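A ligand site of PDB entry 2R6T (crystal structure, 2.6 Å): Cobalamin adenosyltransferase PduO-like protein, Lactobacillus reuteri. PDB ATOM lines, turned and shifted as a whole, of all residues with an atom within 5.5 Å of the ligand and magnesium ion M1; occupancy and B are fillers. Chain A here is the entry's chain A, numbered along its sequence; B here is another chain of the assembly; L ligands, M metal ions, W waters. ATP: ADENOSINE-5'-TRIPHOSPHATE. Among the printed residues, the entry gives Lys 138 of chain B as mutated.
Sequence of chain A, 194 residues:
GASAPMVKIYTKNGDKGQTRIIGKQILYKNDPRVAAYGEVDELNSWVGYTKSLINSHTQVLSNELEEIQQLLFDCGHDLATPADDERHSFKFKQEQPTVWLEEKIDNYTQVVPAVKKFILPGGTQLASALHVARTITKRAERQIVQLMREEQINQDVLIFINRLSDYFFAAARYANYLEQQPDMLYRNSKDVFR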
ATOM      1  N   ILE A   9     -19.959 -11.582  11.269  1.00  0.00           N
ATOM      2  CA  ILE A   9     -19.569 -12.686  10.399  1.00  0.00           C
ATOM      3  C   ILE A   9     -18.601 -13.636  11.132  1.00  0.00           C
ATOM      4  O   ILE A   9     -18.453 -14.800  10.738  1.00  0.00           O
ATOM      5  CB  ILE A   9     -18.986 -12.207   9.050  1.00  0.00           C
ATOM      6  N   TYR A  10     -17.974 -13.125  12.208  1.00  0.00           N
ATOM      7  CA  TYR A  10     -17.070 -13.883  13.081  1.00  0.00           C
ATOM      8  C   TYR A  10     -17.778 -14.402  14.345  1.00  0.00           C
ATOM      9  O   TYR A  10     -18.144 -13.637  15.238  1.00  0.00           O
ATOM     10  CB  TYR A  10     -15.815 -13.054  13.447  1.00  0.00           C
ATOM     11  CG  TYR A  10     -16.058 -11.675  14.042  1.00  0.00           C
ATOM     12  CD1 TYR A  10     -15.897 -11.431  15.420  1.00  0.00           C
ATOM     13  CD2 TYR A  10     -16.446 -10.600  13.236  1.00  0.00           C
ATOM     14  CE1 TYR A  10     -16.129 -10.159  15.975  1.00  0.00           C
ATOM     15  CE2 TYR A  10     -16.690  -9.325  13.778  1.00  0.00           C
ATOM     16  CZ  TYR A  10     -16.522  -9.101  15.144  1.00  0.00           C
ATOM     17  OH  TYR A  10     -16.758  -7.837  15.669  1.00  0.00           O
ATOM     18  N   THR A  11     -17.978 -15.706  14.404  1.00  0.00           N
ATOM     19  CA  THR A  11     -18.627 -16.328  15.555  1.00  0.00           C
ATOM     20  C   THR A  11     -17.622 -16.644  16.667  1.00  0.00           C
ATOM     21  O   THR A  11     -17.999 -16.735  17.838  1.00  0.00           O
ATOM     22  CB  THR A  11     -19.352 -17.633  15.165  1.00  0.00           C
ATOM     23  OG1 THR A  11     -18.392 -18.692  14.959  1.00  0.00           O
ATOM     24  CG2 THR A  11     -20.215 -17.440  13.879  1.00  0.00           C
ATOM     25  N   LYS A  12     -16.336 -16.792  16.310  1.00  0.00           N
ATOM     26  CA  LYS A  12     -15.287 -17.215  17.266  1.00  0.00           C
ATOM     27  C   LYS A  12     -15.360 -18.715  17.658  1.00  0.00           C
ATOM     28  O   LYS A  12     -14.496 -19.231  18.357  1.00  0.00           O
ATOM     29  CB  LYS A  12     -15.238 -16.339  18.532  1.00  0.00           C
ATOM     30  CG  LYS A  12     -15.106 -14.807  18.315  1.00  0.00           C
ATOM     31  CD  LYS A  12     -14.596 -14.142  19.590  1.00  0.00           C
ATOM     32  CE  LYS A  12     -15.087 -12.703  19.745  1.00  0.00           C
ATOM     33  NZ  LYS A  12     -14.845 -12.246  21.152  1.00  0.00           N
ATOM     34  N   ASN A  13     -16.385 -19.419  17.184  1.00  0.00           N
ATOM     35  CA  ASN A  13     -16.485 -20.864  17.328  1.00  0.00           C
ATOM     36  C   ASN A  13     -15.326 -21.675  16.723  1.00  0.00           C
ATOM     37  O   ASN A  13     -15.237 -22.900  16.933  1.00  0.00           O
ATOM     38  CB  ASN A  13     -17.800 -21.360  16.710  1.00  0.00           C
ATOM     39  CG  ASN A  13     -19.032 -20.790  17.410  1.00  0.00           C
ATOM     40  OD1 ASN A  13     -18.979 -20.356  18.576  1.00  0.00           O
ATOM     41  ND2 ASN A  13     -20.155 -20.798  16.697  1.00  0.00           N
ATOM     42  N   GLY A  14     -14.465 -20.998  15.956  1.00  0.00           N
ATOM     43  CA  GLY A  14     -13.412 -21.690  15.233  1.00  0.00           C
ATOM     44  C   GLY A  14     -12.033 -21.454  15.791  1.00  0.00           C
ATOM     45  O   GLY A  14     -11.060 -22.059  15.326  1.00  0.00           O
ATOM     46  N   ASP A  15     -11.953 -20.566  16.792  1.00  0.00           N
ATOM     47  CA  ASP A  15     -10.666 -20.073  17.296  1.00  0.00           C
ATOM     48  C   ASP A  15      -9.788 -21.187  17.874  1.00  0.00           C
ATOM     49  O   ASP A  15      -8.582 -20.985  18.039  1.00  0.00           O
ATOM     50  CB  ASP A  15     -10.879 -18.971  18.330  1.00  0.00           C
ATOM     51  CG  ASP A  15     -11.392 -17.662  17.719  1.00  0.00           C
ATOM     52  OD1 ASP A  15     -11.625 -17.590  16.474  1.00  0.00           O
ATOM     53  OD2 ASP A  15     -11.566 -16.691  18.506  1.00  0.00           O
ATOM     54  N   GLN A  18     -11.444 -25.842  15.236  1.00  0.00           N
ATOM     55  CA  GLN A  18     -12.534 -26.717  14.836  1.00  0.00           C
ATOM     56  C   GLN A  18     -13.616 -25.944  14.117  1.00  0.00           C
ATOM     57  O   GLN A  18     -13.787 -24.740  14.296  1.00  0.00           O
ATOM     58  CB  GLN A  18     -13.126 -27.455  16.040  1.00  0.00           C
ATOM     59  CG  GLN A  18     -12.246 -28.565  16.567  1.00  0.00           C
ATOM     60  CD  GLN A  18     -12.995 -29.498  17.517  1.00  0.00           C
ATOM     61  OE1 GLN A  18     -13.533 -29.069  18.536  1.00  0.00           O
ATOM     62  NE2 GLN A  18     -13.001 -30.783  17.192  1.00  0.00           N
ATOM     63  N   THR A  19     -14.398 -26.659  13.318  1.00  0.00           N
ATOM     64  CA  THR A  19     -15.345 -26.015  12.455  1.00  0.00           C
ATOM     65  C   THR A  19     -16.436 -27.008  12.131  1.00  0.00           C
ATOM     66  O   THR A  19     -16.219 -28.213  12.245  1.00  0.00           O
ATOM     67  CB  THR A  19     -14.635 -25.475  11.189  1.00  0.00           C
ATOM     68  OG1 THR A  19     -15.425 -24.438  10.609  1.00  0.00           O
ATOM     69  CG2 THR A  19     -14.298 -26.589  10.177  1.00  0.00           C
ATOM     70  N   ARG A  20     -17.605 -26.491  11.748  1.00  0.00           N
ATOM     71  CA  ARG A  20     -18.733 -27.314  11.284  1.00  0.00           C
ATOM     72  C   ARG A  20     -18.722 -27.561   9.770  1.00  0.00           C
ATOM     73  O   ARG A  20     -18.275 -26.737   8.980  1.00  0.00           O
ATOM     74  CB  ARG A  20     -20.076 -26.700  11.711  1.00  0.00           C
ATOM     75  CG  ARG A  20     -20.481 -26.934  13.183  1.00  0.00           C
ATOM     76  N   ILE A  21     -19.234 -28.701   9.356  1.00  0.00           N
ATOM     77  CA  ILE A  21     -19.453 -28.983   7.940  1.00  0.00           C
ATOM     78  C   ILE A  21     -20.979 -28.965   7.689  1.00  0.00           C
ATOM     79  O   ILE A  21     -21.753 -28.548   8.565  1.00  0.00           O
ATOM     80  CB  ILE A  21     -18.823 -30.359   7.552  1.00  0.00           C
ATOM     81  CG1 ILE A  21     -19.338 -31.477   8.483  1.00  0.00           C
ATOM     82  CG2 ILE A  21     -17.293 -30.248   7.539  1.00  0.00           C
ATOM     83  CD1 ILE A  21     -19.175 -32.919   7.966  1.00  0.00           C
ATOM     84  N   LYS A  29     -10.001 -28.571  11.346  1.00  0.00           N
ATOM     85  CA  LYS A  29      -9.799 -27.837  10.104  1.00  0.00           C
ATOM     86  C   LYS A  29      -8.769 -28.489   9.166  1.00  0.00           C
ATOM     87  O   LYS A  29      -8.806 -28.251   7.973  1.00  0.00           O
ATOM     88  CB  LYS A  29      -9.480 -26.367  10.387  1.00  0.00           C
ATOM     89  CG  LYS A  29     -10.664 -25.616  10.974  1.00  0.00           C
ATOM     90  CD  LYS A  29     -10.343 -24.193  11.407  1.00  0.00           C
ATOM     91  CE  LYS A  29     -11.642 -23.490  11.781  1.00  0.00           C
ATOM     92  NZ  LYS A  29     -11.492 -22.119  12.301  1.00  0.00           N
ATOM     93  N   VAL A  34     -12.638 -30.875   5.040  1.00  0.00           N
ATOM     94  CA  VAL A  34     -12.377 -29.438   5.090  1.00  0.00           C
ATOM     95  C   VAL A  34     -11.287 -28.996   4.074  1.00  0.00           C
ATOM     96  O   VAL A  34     -11.504 -28.014   3.346  1.00  0.00           O
ATOM     97  CB  VAL A  34     -12.026 -29.012   6.547  1.00  0.00           C
ATOM     98  CG1 VAL A  34     -11.885 -27.517   6.664  1.00  0.00           C
ATOM     99  CG2 VAL A  34     -13.085 -29.509   7.508  1.00  0.00           C
ATOM    100  N   ALA A  35     -10.165 -29.724   3.999  1.00  0.00           N
ATOM    101  CA  ALA A  35      -9.134 -29.486   2.969  1.00  0.00           C
ATOM    102  C   ALA A  35      -9.685 -29.538   1.523  1.00  0.00           C
ATOM    103  O   ALA A  35      -9.438 -28.622   0.733  1.00  0.00           O
ATOM    104  CB  ALA A  35      -7.964 -30.446   3.120  1.00  0.00           C
ATOM    105  N   TYR A  37     -13.030 -29.227   0.401  1.00  0.00           N
ATOM    106  CA  TYR A  37     -13.960 -28.097   0.266  1.00  0.00           C
ATOM    107  C   TYR A  37     -13.137 -26.787   0.240  1.00  0.00           C
ATOM    108  O   TYR A  37     -13.435 -25.854  -0.538  1.00  0.00           O
ATOM    109  CB  TYR A  37     -14.987 -28.129   1.416  1.00  0.00           C
ATOM    110  CG  TYR A  37     -15.798 -26.864   1.631  1.00  0.00           C
ATOM    111  N   GLY A  38     -12.087 -26.739   1.061  1.00  0.00           N
ATOM    112  CA  GLY A  38     -11.147 -25.603   1.103  1.00  0.00           C
ATOM    113  C   GLY A  38     -10.344 -25.307  -0.166  1.00  0.00           C
ATOM    114  O   GLY A  38     -10.296 -24.147  -0.587  1.00  0.00           O
ATOM    115  N   LYS B 138      -7.041 -19.426   5.086  1.00  0.00           N
ATOM    116  CA  LYS B 138      -7.645 -20.680   5.532  1.00  0.00           C
ATOM    117  C   LYS B 138      -6.737 -21.907   5.347  1.00  0.00           C
ATOM    118  O   LYS B 138      -6.633 -22.772   6.236  1.00  0.00           O
ATOM    119  CB  LYS B 138      -8.959 -20.930   4.815  1.00  0.00           C
ATOM    120  CG  LYS B 138     -10.094 -19.999   5.157  1.00  0.00           C
ATOM    121  CD  LYS B 138     -11.242 -20.311   4.211  1.00  0.00           C
ATOM    122  N   ARG B 139      -6.089 -21.980   4.187  1.00  0.00           N
ATOM    123  CA  ARG B 139      -5.098 -23.019   3.915  1.00  0.00           C
ATOM    124  C   ARG B 139      -3.966 -23.044   4.949  1.00  0.00           C
ATOM    125  O   ARG B 139      -3.602 -24.135   5.470  1.00  0.00           O
ATOM    126  CB  ARG B 139      -4.560 -22.878   2.468  1.00  0.00           C
ATOM    127  CG  ARG B 139      -3.368 -23.739   2.155  1.00  0.00           C
ATOM    128  CD  ARG B 139      -3.322 -24.168   0.704  1.00  0.00           C
ATOM    129  NE  ARG B 139      -3.176 -23.066  -0.249  1.00  0.00           N
ATOM    130  CZ  ARG B 139      -2.040 -22.450  -0.544  1.00  0.00           C
ATOM    131  NH1 ARG B 139      -0.907 -22.797   0.036  1.00  0.00           N
ATOM    132  NH2 ARG B 139      -2.032 -21.480  -1.448  1.00  0.00           N
ATOM    133  N   GLU B 141      -4.216 -21.809   7.864  1.00  0.00           N
ATOM    134  CA  GLU B 141      -4.901 -22.131   9.117  1.00  0.00           C
ATOM    135  C   GLU B 141      -5.075 -23.633   9.311  1.00  0.00           C
ATOM    136  O   GLU B 141      -4.847 -24.130  10.410  1.00  0.00           O
ATOM    137  CB  GLU B 141      -6.252 -21.416   9.216  1.00  0.00           C
ATOM    138  CG  GLU B 141      -6.890 -21.553  10.606  1.00  0.00           C
ATOM    139  CD  GLU B 141      -8.339 -21.162  10.654  1.00  0.00           C
ATOM    140  OE1 GLU B 141      -8.928 -20.964   9.570  1.00  0.00           O
ATOM    141  OE2 GLU B 141      -8.890 -21.067  11.783  1.00  0.00           O
ATOM    142  N   ARG B 142      -5.491 -24.346   8.268  1.00  0.00           N
ATOM    143  CA  ARG B 142      -5.584 -25.801   8.321  1.00  0.00           C
ATOM    144  C   ARG B 142      -4.250 -26.426   8.684  1.00  0.00           C
ATOM    145  O   ARG B 142      -4.190 -27.374   9.502  1.00  0.00           O
ATOM    146  CB  ARG B 142      -6.021 -26.347   6.981  1.00  0.00           C
ATOM    147  CG  ARG B 142      -7.433 -26.026   6.635  1.00  0.00           C
ATOM    148  CD  ARG B 142      -7.891 -26.855   5.469  1.00  0.00           C
ATOM    149  NE  ARG B 142      -7.132 -26.603   4.248  1.00  0.00           N
ATOM    150  CZ  ARG B 142      -7.420 -25.624   3.391  1.00  0.00           C
ATOM    151  NH1 ARG B 142      -8.430 -24.798   3.647  1.00  0.00           N
ATOM    152  NH2 ARG B 142      -6.729 -25.485   2.279  1.00  0.00           N
ATOM    153  N   ASN B 162      -7.571 -17.135  12.192  1.00  0.00           N
ATOM    154  CA  ASN B 162      -8.982 -17.402  12.020  1.00  0.00           C
ATOM    155  C   ASN B 162      -9.752 -16.107  11.716  1.00  0.00           C
ATOM    156  O   ASN B 162     -10.464 -16.018  10.700  1.00  0.00           O
ATOM    157  CB  ASN B 162      -9.541 -18.124  13.245  1.00  0.00           C
ATOM    158  CG  ASN B 162     -11.002 -18.487  13.096  1.00  0.00           C
ATOM    159  OD1 ASN B 162     -11.506 -18.677  11.971  1.00  0.00           O
ATOM    160  ND2 ASN B 162     -11.708 -18.565  14.231  1.00  0.00           N
ATOM    161  N   ARG B 163      -9.581 -15.106  12.567  1.00  0.00           N
ATOM    162  CA  ARG B 163     -10.229 -13.819  12.331  1.00  0.00           C
ATOM    163  C   ARG B 163      -9.776 -13.167  11.025  1.00  0.00           C
ATOM    164  O   ARG B 163     -10.581 -12.463  10.410  1.00  0.00           O
ATOM    165  CB  ARG B 163      -9.988 -12.856  13.507  1.00  0.00           C
ATOM    166  CG  ARG B 163     -11.041 -11.782  13.635  1.00  0.00           C
ATOM    167  CD  ARG B 163     -12.321 -12.346  14.234  1.00  0.00           C
ATOM    168  NE  ARG B 163     -12.137 -12.803  15.627  1.00  0.00           N
ATOM    169  CZ  ARG B 163     -12.051 -14.075  16.024  1.00  0.00           C
ATOM    170  NH1 ARG B 163     -12.122 -15.065  15.160  1.00  0.00           N
ATOM    171  NH2 ARG B 163     -11.879 -14.354  17.305  1.00  0.00           N
ATOM    172  N   SER B 165      -9.043 -14.384   7.954  1.00  0.00           N
ATOM    173  CA  SER B 165      -9.808 -14.759   6.754  1.00  0.00           C
ATOM    174  C   SER B 165     -11.165 -14.066   6.688  1.00  0.00           C
ATOM    175  O   SER B 165     -11.643 -13.747   5.578  1.00  0.00           O
ATOM    176  CB  SER B 165      -9.957 -16.281   6.595  1.00  0.00           C
ATOM    177  OG  SER B 165     -10.556 -16.850   7.728  1.00  0.00           O
ATOM    178  N   ASP B 166     -11.767 -13.832   7.855  1.00  0.00           N
ATOM    179  CA  ASP B 166     -13.007 -13.055   8.003  1.00  0.00           C
ATOM    180  C   ASP B 166     -12.776 -11.590   7.595  1.00  0.00           C
ATOM    181  O   ASP B 166     -13.574 -11.025   6.852  1.00  0.00           O
ATOM    182  CB  ASP B 166     -13.534 -13.115   9.445  1.00  0.00           C
ATOM    183  CG  ASP B 166     -14.343 -14.361   9.740  1.00  0.00           C
ATOM    184  OD1 ASP B 166     -14.536 -15.231   8.855  1.00  0.00           O
ATOM    185  OD2 ASP B 166     -14.806 -14.463  10.885  1.00  0.00           O
HETATM  186  PG  ATP L   1     -15.440 -18.575  12.830  1.00  0.00           P
HETATM  187  O1G ATP L   1     -16.715 -17.790  13.014  1.00  0.00           O
HETATM  188  O2G ATP L   1     -14.830 -19.008  14.158  1.00  0.00           O
HETATM  189  O3G ATP L   1     -14.471 -17.945  11.846  1.00  0.00           O
HETATM  190  PB  ATP L   1     -15.225 -21.200  11.564  1.00  0.00           P
HETATM  191  O1B ATP L   1     -13.758 -20.952  11.774  1.00  0.00           O
HETATM  192  O2B ATP L   1     -15.794 -22.447  12.167  1.00  0.00           O
HETATM  193  O3B ATP L   1     -16.033 -19.916  12.127  1.00  0.00           O
HETATM  194  PA  ATP L   1     -15.870 -19.899   9.008  1.00  0.00           P
HETATM  195  O1A ATP L   1     -14.601 -19.101   9.079  1.00  0.00           O
HETATM  196  O2A ATP L   1     -17.201 -19.274   9.318  1.00  0.00           O
HETATM  197  O3A ATP L   1     -15.612 -21.183   9.985  1.00  0.00           O
HETATM  198  O5' ATP L   1     -15.960 -20.525   7.504  1.00  0.00           O
HETATM  199  C5' ATP L   1     -17.164 -20.921   6.862  1.00  0.00           C
HETATM  200  C4' ATP L   1     -17.179 -22.434   6.590  1.00  0.00           C
HETATM  201  O4' ATP L   1     -16.047 -22.842   5.802  1.00  0.00           O
HETATM  202  C3' ATP L   1     -17.095 -23.280   7.867  1.00  0.00           C
HETATM  203  O3' ATP L   1     -18.355 -23.740   8.311  1.00  0.00           O
HETATM  204  C2' ATP L   1     -16.244 -24.480   7.507  1.00  0.00           C
HETATM  205  O2' ATP L   1     -17.043 -25.542   6.985  1.00  0.00           O
HETATM  206  C1' ATP L   1     -15.360 -23.975   6.390  1.00  0.00           C
HETATM  207  N9  ATP L   1     -14.037 -23.629   6.959  1.00  0.00           N
HETATM  208  C8  ATP L   1     -13.775 -23.069   8.151  1.00  0.00           C
HETATM  209  N7  ATP L   1     -12.441 -22.900   8.364  1.00  0.00           N
HETATM  210  C5  ATP L   1     -11.814 -23.370   7.271  1.00  0.00           C
HETATM  211  C6  ATP L   1     -10.420 -23.489   6.816  1.00  0.00           C
HETATM  212  N6  ATP L   1      -9.408 -23.064   7.581  1.00  0.00           N
HETATM  213  N1  ATP L   1     -10.200 -24.052   5.602  1.00  0.00           N
HETATM  214  C2  ATP L   1     -11.207 -24.485   4.806  1.00  0.00           C
HETATM  215  N3  ATP L   1     -12.497 -24.401   5.156  1.00  0.00           N
HETATM  216  C4  ATP L   1     -12.872 -23.860   6.352  1.00  0.00           C
HETATM  217 MG    MG M   1     -12.915 -19.365  10.723  1.00  0.00          MG
HETATM  218 MG    MG M   2     -16.391 -16.728  10.348  1.00  0.00          MG
HETATM  219  O   HOH W   1     -11.772 -20.421   9.414  1.00  0.00           O
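An oxygen (O2G) of the ligand sits at hydrogen-bond distance from the backbone NH (N) of Asn 13, 3.4 Å away.
The backbone NH of Lys 12 is in hydrogen-bond range of an oxygen (O2G) of the ligand.
The side-chain hydroxyl (OG1) of Thr 19 sits at hydrogen-bond distance from an oxygen (O2B) of the ligand (2.6 Å).
An oxygen (O1B) of the ligand sits close to the side-chain amino group (NZ) of Lys 29, at 2.6 Å.
The backbone carbonyl oxygen of Lys 138 of chain B is in hydrogen-bond range of a nitrogen (N6) of the ligand, 3.1 Å away.
An oxygen (O2G) of the ligand lies within hydrogen-bond range of the backbone NH of Gly 14, 2.7 Å away.
The side-chain carboxylate (OE1) of Glu 141 of chain B sits at hydrogen-bond distance from a nitrogen (N6) of the ligand.
The backbone carbonyl oxygen (O) of Arg 20 lies within hydrogen-bond range of an oxygen (O2') of the ligand, 2.6 Å away.
The side-chain hydroxyl (OG1) of Thr 11 is in hydrogen-bond range of an oxygen (O1G) of the ligand, at 2.7 Å.
N1 of the ligand is in hydrogen-bond range of NH1 of Arg 142 of chain B, 2.7 Å away.
An oxygen (O1G) of the ligand is in hydrogen-bond range of the backbone NH of Thr 11 (2.8 Å).
Residues that only touch magnesium ion M1: Lys 29.
Of the 24 residues printed, 2 come within 4 Å of magnesium ion M1.
The nearest printed residue that does not touch magnesium ion M1 is Glu 141 of chain B (4.4 Å).
C of Tyr 10 touches O1G of the ligand, 3.8 Å away.
O of Gln 18 touches O2B of the ligand (3.7 Å).
Val 34 touches the ligand.
Gly 38 touches the ligand (CA to C2, 3.9 Å).
Asp 166 of chain B touches the ligand (OD2 to O3G, 3.6 Å).
Magnesium ion M1 is bound by OD1 of Asn 162 of chain B (2.0 Å), water W1 (2.0 Å), O1B of the ligand (2.1 Å), O1A of the ligand (2.4 Å) and O3G of the ligand (2.4 Å).
ND2 of Asn 162 of chain B lies within hydrogen-bond range of OD1 of Asp 15.
The side-chain amino group (NZ) of Lys 29 lies close to the side-chain amide oxygen (OD1) of Asn 162 of chain B (3.5 Å).
The side-chain hydroxyl (OG1) of Thr 11 sits close to the backbone NH (N) of Asn 13 (3.1 Å).
NZ of Lys 29 is in hydrogen-bond range of O of Gly 14.
NZ of Lys 29 lies within salt-bridge range of OE2 of Glu 141 of chain B.
The side-chain hydroxyl (OG) of Ser 165 of chain B is in hydrogen-bond range of the backbone carbonyl oxygen (O) of Asn 162 of chain B.
Water W1 lies within hydrogen-bond range of N7 of the ligand (2.8 Å), OE1 of Glu 141 of chain B (2.9 Å) and NZ of Lys 29 (3.4 Å).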
